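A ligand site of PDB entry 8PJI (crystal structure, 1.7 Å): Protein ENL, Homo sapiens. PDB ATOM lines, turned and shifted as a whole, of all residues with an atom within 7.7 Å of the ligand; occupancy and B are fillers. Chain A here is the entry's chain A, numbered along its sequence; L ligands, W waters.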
ATOM      1  N   GLU A  26       5.053  15.614   2.075  1.00  0.00           N
ATOM      2  CA  GLU A  26       5.372  14.324   2.750  1.00  0.00           C
ATOM      3  C   GLU A  26       4.082  13.550   3.020  1.00  0.00           C
ATOM      4  O   GLU A  26       4.186  12.411   3.496  1.00  0.00           O
ATOM      5  CB  GLU A  26       6.123  14.524   4.074  1.00  0.00           C
ATOM      6  CG  GLU A  26       7.442  15.256   3.929  1.00  0.00           C
ATOM      7  CD  GLU A  26       7.398  16.759   4.199  1.00  0.00           C
ATOM      8  OE1 GLU A  26       6.321  17.284   4.652  1.00  0.00           O
ATOM      9  OE2 GLU A  26       8.437  17.395   3.979  1.00  0.00           O
ATOM     10  N   PHE A  28       1.783  14.871   5.352  1.00  0.00           N
ATOM     11  CA  PHE A  28       1.352  15.249   6.715  1.00  0.00           C
ATOM     12  C   PHE A  28       0.049  16.039   6.615  1.00  0.00           C
ATOM     13  O   PHE A  28      -0.025  17.028   5.886  1.00  0.00           O
ATOM     14  CB  PHE A  28       2.417  16.058   7.458  1.00  0.00           C
ATOM     15  CG  PHE A  28       3.755  15.367   7.543  1.00  0.00           C
ATOM     16  CD1 PHE A  28       3.841  13.987   7.464  1.00  0.00           C
ATOM     17  CD2 PHE A  28       4.922  16.104   7.621  1.00  0.00           C
ATOM     18  CE1 PHE A  28       5.070  13.353   7.506  1.00  0.00           C
ATOM     19  CE2 PHE A  28       6.153  15.475   7.672  1.00  0.00           C
ATOM     20  CZ  PHE A  28       6.223  14.113   7.630  1.00  0.00           C
ATOM     21  N   THR A  29      -0.948  15.566   7.327  1.00  0.00           N
ATOM     22  CA  THR A  29      -2.338  16.062   7.255  1.00  0.00           C
ATOM     23  C   THR A  29      -2.619  17.161   8.271  1.00  0.00           C
ATOM     24  O   THR A  29      -3.653  17.847   8.118  1.00  0.00           O
ATOM     25  CB  THR A  29      -3.266  14.871   7.489  1.00  0.00           C
ATOM     26  OG1 THR A  29      -2.891  14.305   8.752  1.00  0.00           O
ATOM     27  CG2 THR A  29      -3.129  13.839   6.395  1.00  0.00           C
ATOM     28  N   HIS A  30      -1.802  17.297   9.323  1.00  0.00           N
ATOM     29  CA  HIS A  30      -2.142  18.137  10.504  1.00  0.00           C
ATOM     30  C   HIS A  30      -0.984  19.047  10.855  1.00  0.00           C
ATOM     31  O   HIS A  30       0.222  18.669  10.638  1.00  0.00           O
ATOM     32  CB  HIS A  30      -2.500  17.311  11.736  1.00  0.00           C
ATOM     33  CG  HIS A  30      -3.834  16.647  11.717  1.00  0.00           C
ATOM     34  ND1 HIS A  30      -4.045  15.443  11.063  1.00  0.00           N
ATOM     35  CD2 HIS A  30      -4.990  16.962  12.346  1.00  0.00           C
ATOM     36  CE1 HIS A  30      -5.305  15.080  11.281  1.00  0.00           C
ATOM     37  NE2 HIS A  30      -5.908  15.987  12.038  1.00  0.00           N
ATOM     38  N   TRP A  32       0.323  20.926  14.420  1.00  0.00           N
ATOM     39  CA  TRP A  32       0.043  20.835  15.882  1.00  0.00           C
ATOM     40  C   TRP A  32       1.112  21.595  16.641  1.00  0.00           C
ATOM     41  O   TRP A  32       2.238  21.884  16.088  1.00  0.00           O
ATOM     42  CB  TRP A  32      -0.147  19.385  16.350  1.00  0.00           C
ATOM     43  CG  TRP A  32       0.994  18.428  16.182  1.00  0.00           C
ATOM     44  CD1 TRP A  32       1.037  17.393  15.286  1.00  0.00           C
ATOM     45  CD2 TRP A  32       2.198  18.312  16.973  1.00  0.00           C
ATOM     46  NE1 TRP A  32       2.189  16.684  15.415  1.00  0.00           N
ATOM     47  CE2 TRP A  32       2.930  17.215  16.448  1.00  0.00           C
ATOM     48  CE3 TRP A  32       2.735  19.025  18.042  1.00  0.00           C
ATOM     49  CZ2 TRP A  32       4.164  16.827  16.951  1.00  0.00           C
ATOM     50  CZ3 TRP A  32       3.968  18.646  18.541  1.00  0.00           C
ATOM     51  CH2 TRP A  32       4.661  17.547  18.021  1.00  0.00           C
ATOM     52  N   LEU A  55       9.475  13.785  21.541  1.00  0.00           N
ATOM     53  CA  LEU A  55       8.607  13.489  20.377  1.00  0.00           C
ATOM     54  C   LEU A  55       8.722  12.004  20.042  1.00  0.00           C
ATOM     55  O   LEU A  55       9.698  11.367  20.440  1.00  0.00           O
ATOM     56  CB  LEU A  55       9.033  14.370  19.211  1.00  0.00           C
ATOM     57  CG  LEU A  55       8.282  15.698  19.144  1.00  0.00           C
ATOM     58  CD1 LEU A  55       8.367  16.454  20.462  1.00  0.00           C
ATOM     59  CD2 LEU A  55       8.791  16.538  17.991  1.00  0.00           C
ATOM     60  N   HIS A  56       7.725  11.469  19.343  1.00  0.00           N
ATOM     61  CA  HIS A  56       7.793  10.096  18.764  1.00  0.00           C
ATOM     62  C   HIS A  56       9.120   9.903  18.011  1.00  0.00           C
ATOM     63  O   HIS A  56       9.587  10.860  17.386  1.00  0.00           O
ATOM     64  CB  HIS A  56       6.587   9.884  17.882  1.00  0.00           C
ATOM     65  CG  HIS A  56       6.388   8.464  17.478  1.00  0.00           C
ATOM     66  ND1 HIS A  56       6.931   7.956  16.314  1.00  0.00           N
ATOM     67  CD2 HIS A  56       5.694   7.468  18.058  1.00  0.00           C
ATOM     68  CE1 HIS A  56       6.565   6.690  16.200  1.00  0.00           C
ATOM     69  NE2 HIS A  56       5.790   6.381  17.244  1.00  0.00           N
ATOM     70  N   ASP A  57       9.735   8.721  18.080  1.00  0.00           N
ATOM     71  CA  ASP A  57      11.049   8.426  17.433  1.00  0.00           C
ATOM     72  C   ASP A  57      11.002   8.778  15.929  1.00  0.00           C
ATOM     73  O   ASP A  57      12.076   8.987  15.347  1.00  0.00           O
ATOM     74  CB  ASP A  57      11.416   6.952  17.605  1.00  0.00           C
ATOM     75  CG  ASP A  57      11.419   6.428  19.038  1.00  0.00           C
ATOM     76  OD1 ASP A  57      11.560   7.226  19.966  1.00  0.00           O
ATOM     77  OD2 ASP A  57      11.284   5.195  19.225  1.00  0.00           O
ATOM     78  N   SER A  58       9.833   8.813  15.296  1.00  0.00           N
ATOM     79  CA  SER A  58       9.713   9.053  13.830  1.00  0.00           C
ATOM     80  C   SER A  58      10.101  10.500  13.480  1.00  0.00           C
ATOM     81  O   SER A  58      10.340  10.775  12.276  1.00  0.00           O
ATOM     82  CB  SER A  58       8.337   8.712  13.285  1.00  0.00           C
ATOM     83  OG  SER A  58       7.333   9.562  13.834  1.00  0.00           O
ATOM     84  N   PHE A  59      10.102  11.419  14.448  1.00  0.00           N
ATOM     85  CA  PHE A  59      10.421  12.830  14.173  1.00  0.00           C
ATOM     86  C   PHE A  59      11.928  13.003  14.162  1.00  0.00           C
ATOM     87  O   PHE A  59      12.625  12.298  14.863  1.00  0.00           O
ATOM     88  CB  PHE A  59       9.807  13.751  15.224  1.00  0.00           C
ATOM     89  CG  PHE A  59       8.333  13.957  15.061  1.00  0.00           C
ATOM     90  CD1 PHE A  59       7.435  13.040  15.575  1.00  0.00           C
ATOM     91  CD2 PHE A  59       7.847  15.029  14.357  1.00  0.00           C
ATOM     92  CE1 PHE A  59       6.075  13.234  15.429  1.00  0.00           C
ATOM     93  CE2 PHE A  59       6.475  15.199  14.191  1.00  0.00           C
ATOM     94  CZ  PHE A  59       5.608  14.293  14.719  1.00  0.00           C
ATOM     95  N   PRO A  60      12.471  13.918  13.344  1.00  0.00           N
ATOM     96  CA  PRO A  60      13.887  14.266  13.440  1.00  0.00           C
ATOM     97  C   PRO A  60      14.158  14.972  14.776  1.00  0.00           C
ATOM     98  O   PRO A  60      13.274  15.627  15.260  1.00  0.00           O
ATOM     99  CB  PRO A  60      14.116  15.205  12.252  1.00  0.00           C
ATOM    100  CG  PRO A  60      12.751  15.767  11.943  1.00  0.00           C
ATOM    101  CD  PRO A  60      11.777  14.660  12.296  1.00  0.00           C
ATOM    102  N   ARG A  64      13.322  17.542  22.090  1.00  0.00           N
ATOM    103  CA  ARG A  64      13.202  18.983  21.790  1.00  0.00           C
ATOM    104  C   ARG A  64      13.297  19.753  23.111  1.00  0.00           C
ATOM    105  O   ARG A  64      12.494  19.477  24.035  1.00  0.00           O
ATOM    106  CB  ARG A  64      11.871  19.236  21.063  1.00  0.00           C
ATOM    107  CG  ARG A  64      11.750  18.531  19.720  1.00  0.00           C
ATOM    108  CD  ARG A  64      12.644  19.131  18.659  1.00  0.00           C
ATOM    109  NE  ARG A  64      12.434  18.358  17.458  1.00  0.00           N
ATOM    110  CZ  ARG A  64      11.473  18.559  16.543  1.00  0.00           C
ATOM    111  NH1 ARG A  64      10.632  19.573  16.631  1.00  0.00           N
ATOM    112  NH2 ARG A  64      11.369  17.731  15.512  1.00  0.00           N
ATOM    113  N   GLU A  74       6.274  23.430  17.690  1.00  0.00           N
ATOM    114  CA  GLU A  74       5.326  23.490  16.541  1.00  0.00           C
ATOM    115  C   GLU A  74       5.750  22.416  15.542  1.00  0.00           C
ATOM    116  O   GLU A  74       6.949  22.369  15.218  1.00  0.00           O
ATOM    117  CB  GLU A  74       5.287  24.920  16.020  1.00  0.00           C
ATOM    118  CG  GLU A  74       4.758  25.841  17.096  1.00  0.00           C
ATOM    119  CD  GLU A  74       4.512  27.286  16.764  1.00  0.00           C
ATOM    120  OE1 GLU A  74       5.335  27.873  16.065  1.00  0.00           O
ATOM    121  OE2 GLU A  74       3.502  27.833  17.266  1.00  0.00           O
ATOM    122  N   GLU A  75       4.825  21.563  15.143  1.00  0.00           N
ATOM    123  CA  GLU A  75       5.155  20.469  14.188  1.00  0.00           C
ATOM    124  C   GLU A  75       4.052  20.224  13.163  1.00  0.00           C
ATOM    125  O   GLU A  75       2.936  20.733  13.328  1.00  0.00           O
ATOM    126  CB  GLU A  75       5.424  19.158  14.940  1.00  0.00           C
ATOM    127  CG  GLU A  75       6.891  18.883  15.188  1.00  0.00           C
ATOM    128  CD  GLU A  75       7.786  18.781  13.960  1.00  0.00           C
ATOM    129  OE1 GLU A  75       7.267  18.591  12.857  1.00  0.00           O
ATOM    130  OE2 GLU A  75       9.025  18.896  14.106  1.00  0.00           O
ATOM    131  N   SER A  76       4.396  19.415  12.160  1.00  0.00           N
ATOM    132  CA  SER A  76       3.436  18.812  11.206  1.00  0.00           C
ATOM    133  C   SER A  76       3.519  17.291  11.288  1.00  0.00           C
ATOM    134  O   SER A  76       4.612  16.760  11.542  1.00  0.00           O
ATOM    135  CB  SER A  76       3.690  19.311   9.803  1.00  0.00           C
ATOM    136  OG  SER A  76       3.103  20.599   9.670  1.00  0.00           O
ATOM    137  N   GLY A  77       2.396  16.619  11.110  1.00  0.00           N
ATOM    138  CA  GLY A  77       2.383  15.162  11.098  1.00  0.00           C
ATOM    139  C   GLY A  77       1.030  14.593  10.739  1.00  0.00           C
ATOM    140  O   GLY A  77       0.175  15.339  10.287  1.00  0.00           O
ATOM    141  N   TYR A  78       0.879  13.297  10.940  1.00  0.00           N
ATOM    142  CA  TYR A  78      -0.301  12.537  10.472  1.00  0.00           C
ATOM    143  C   TYR A  78      -0.866  11.652  11.576  1.00  0.00           C
ATOM    144  O   TYR A  78      -1.861  10.990  11.308  1.00  0.00           O
ATOM    145  CB  TYR A  78       0.100  11.737   9.226  1.00  0.00           C
ATOM    146  CG  TYR A  78       1.239  10.770   9.411  1.00  0.00           C
ATOM    147  CD1 TYR A  78       2.557  11.174   9.255  1.00  0.00           C
ATOM    148  CD2 TYR A  78       1.004   9.449   9.729  1.00  0.00           C
ATOM    149  CE1 TYR A  78       3.611  10.298   9.434  1.00  0.00           C
ATOM    150  CE2 TYR A  78       2.041   8.560   9.929  1.00  0.00           C
ATOM    151  CZ  TYR A  78       3.347   8.976   9.756  1.00  0.00           C
ATOM    152  OH  TYR A  78       4.369   8.089   9.922  1.00  0.00           O
ATOM    153  N   ALA A  79      -0.294  11.620  12.788  1.00  0.00           N
ATOM    154  CA  ALA A  79      -0.876  10.769  13.852  1.00  0.00           C
ATOM    155  C   ALA A  79      -0.603  11.356  15.244  1.00  0.00           C
ATOM    156  O   ALA A  79       0.473  11.973  15.436  1.00  0.00           O
ATOM    157  CB  ALA A  79      -0.360   9.355  13.730  1.00  0.00           C
ATOM    158  N   GLY A  80      -1.528  11.139  16.172  1.00  0.00           N
ATOM    159  CA  GLY A  80      -1.338  11.389  17.615  1.00  0.00           C
ATOM    160  C   GLY A  80      -0.324  10.419  18.211  1.00  0.00           C
ATOM    161  O   GLY A  80      -0.006   9.375  17.554  1.00  0.00           O
ATOM    162  N   PHE A  81       0.156  10.710  19.423  1.00  0.00           N
ATOM    163  CA  PHE A  81       1.070   9.825  20.190  1.00  0.00           C
ATOM    164  C   PHE A  81       1.160  10.340  21.633  1.00  0.00           C
ATOM    165  O   PHE A  81       0.725  11.478  21.904  1.00  0.00           O
ATOM    166  CB  PHE A  81       2.471   9.757  19.565  1.00  0.00           C
ATOM    167  CG  PHE A  81       3.161  11.091  19.405  1.00  0.00           C
ATOM    168  CD1 PHE A  81       2.948  11.862  18.273  1.00  0.00           C
ATOM    169  CD2 PHE A  81       3.997  11.597  20.395  1.00  0.00           C
ATOM    170  CE1 PHE A  81       3.613  13.064  18.110  1.00  0.00           C
ATOM    171  CE2 PHE A  81       4.633  12.816  20.249  1.00  0.00           C
ATOM    172  CZ  PHE A  81       4.420  13.560  19.108  1.00  0.00           C
ATOM    173  N   ILE A  82       1.722   9.516  22.500  1.00  0.00           N
ATOM    174  CA  ILE A  82       1.919   9.834  23.938  1.00  0.00           C
ATOM    175  C   ILE A  82       3.292  10.503  24.019  1.00  0.00           C
ATOM    176  O   ILE A  82       4.253   9.917  23.522  1.00  0.00           O
ATOM    177  CB  ILE A  82       1.819   8.580  24.805  1.00  0.00           C
ATOM    178  CG1 ILE A  82       0.446   7.917  24.651  1.00  0.00           C
ATOM    179  CG2 ILE A  82       2.090   8.934  26.272  1.00  0.00           C
ATOM    180  CD1 ILE A  82      -0.716   8.852  24.950  1.00  0.00           C
ATOM    181  N   LEU A 104      -0.899  13.602  23.025  1.00  0.00           N
ATOM    182  CA  LEU A 104      -0.991  14.529  21.859  1.00  0.00           C
ATOM    183  C   LEU A 104      -1.915  13.913  20.792  1.00  0.00           C
ATOM    184  O   LEU A 104      -1.394  13.226  19.931  1.00  0.00           O
ATOM    185  CB  LEU A 104       0.368  14.855  21.246  1.00  0.00           C
ATOM    186  CG  LEU A 104       0.265  16.087  20.359  1.00  0.00           C
ATOM    187  CD1 LEU A 104       0.939  17.291  21.004  1.00  0.00           C
ATOM    188  CD2 LEU A 104       0.767  15.843  18.956  1.00  0.00           C
ATOM    189  N   LEU A 106      -4.866  14.140  17.679  1.00  0.00           N
ATOM    190  CA  LEU A 106      -5.249  14.956  16.495  1.00  0.00           C
ATOM    191  C   LEU A 106      -6.756  14.797  16.221  1.00  0.00           C
ATOM    192  O   LEU A 106      -7.315  13.824  16.691  1.00  0.00           O
ATOM    193  CB  LEU A 106      -4.438  14.471  15.299  1.00  0.00           C
ATOM    194  CG  LEU A 106      -2.928  14.478  15.486  1.00  0.00           C
ATOM    195  CD1 LEU A 106      -2.246  14.090  14.180  1.00  0.00           C
ATOM    196  CD2 LEU A 106      -2.442  15.824  15.968  1.00  0.00           C
HETATM  197  N1  LIG L   1       4.692  10.644  12.893  1.00  0.00           N
HETATM  198  N2  LIG L   1       6.899  11.520  11.530  1.00  0.00           N
HETATM  199  C1  LIG L   1       2.922   8.992  15.689  1.00  0.00           C
HETATM  200  C2  LIG L   1       3.205   7.821  14.749  1.00  0.00           C
HETATM  201  C3  LIG L   1       4.575  11.849  12.335  1.00  0.00           C
HETATM  202  C4  LIG L   1       5.818  12.369  11.741  1.00  0.00           C
HETATM  203  C5  LIG L   1       6.134  13.639  11.337  1.00  0.00           C
HETATM  204  C6  LIG L   1       8.198  14.676  10.373  1.00  0.00           C
HETATM  205  C7  LIG L   1       9.750  16.798   9.477  1.00  0.00           C
HETATM  206  C8  LIG L   1       9.273  14.434   9.539  1.00  0.00           C
HETATM  207  C9  LIG L   1       3.744   8.414  13.456  1.00  0.00           C
HETATM  208  C10 LIG L   1       3.619   9.943  13.582  1.00  0.00           C
HETATM  209  C11 LIG L   1       3.682  10.161  15.117  1.00  0.00           C
HETATM  210  O1  LIG L   1       3.515  12.494  12.278  1.00  0.00           O
HETATM  211  N3  LIG L   1       7.438  13.581  10.892  1.00  0.00           N
HETATM  212  C12 LIG L   1       7.845  12.278  11.031  1.00  0.00           C
HETATM  213  C13 LIG L   1       7.908  15.979  10.787  1.00  0.00           C
HETATM  214  C14 LIG L   1       8.700  17.025  10.340  1.00  0.00           C
HETATM  215  C15 LIG L   1      10.010  15.494   9.067  1.00  0.00           C
HETATM  216  O2  LIG L   1       8.482  18.304  10.758  1.00  0.00           O
HETATM  217  O   HOH W   1       6.776   9.109  10.119  1.00  0.00           O
HETATM  218  O   HOH W   2       2.260  13.872  14.360  1.00  0.00           O
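The side-chain hydroxyl (OG) of Ser 58 sits at hydrogen-bond distance from a nitrogen (N1) of the ligand, at 3.0 Å. The side-chain carboxylate (OE1) of Glu 75 lies within hydrogen-bond range of an oxygen (O2) of the ligand. N of Tyr 78 is in hydrogen-bond range of O1 of the ligand, at 3.1 Å.
The guanidinium group (NH2) of Arg 64 is in hydrogen-bond range of the backbone carbonyl oxygen (O) of Pro 60 (2.8 Å). OE2 of Glu 75 lies within salt-bridge range of NH2 of Arg 64. N of Glu 75 is in hydrogen-bond range of O of Trp 32, at 2.8 Å. O of Gly 77 lies within hydrogen-bond range of N of Thr 29 (3.2 Å). A ring nitrogen (ND1) of His 56 is in hydrogen-bond range of the side-chain hydroxyl (OG) of Ser 58, at 3.0 Å. The backbone carbonyl oxygen of Gly 77 is in hydrogen-bond range of the backbone NH of His 30, at 2.9 Å. O of Phe 81 sits at hydrogen-bond distance from N of Leu 104 (2.9 Å).
Phe 28 touches the ligand. His 56 touches the ligand. Phe 59 touches the ligand (CE2 to C5, 3.3 Å). Pro 60 touches the ligand. O of Ser 76 touches C13 of the ligand (3.5 Å). CA of Gly 77 touches O1 of the ligand, at 3.1 Å. O of Ala 79 touches C11 of the ligand, at 3.7 Å. O of Gly 80 touches C1 of the ligand (3.5 Å). Phe 81 touches the ligand (CD1 to C11, 3.7 Å). Hydrophobic or aromatic side chains that line the ligand: Phe 28, His 56, Phe 59, Pro 60, Tyr 78, Ala 79 and Phe 81.
Water W2 lies within hydrogen-bond range of O1 of the ligand, O of Ala 79 and NE1 of Trp 32. Water W1 bridges the side-chain hydroxyl (OH) of Tyr 78 and a nitrogen (N2) of the ligand.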
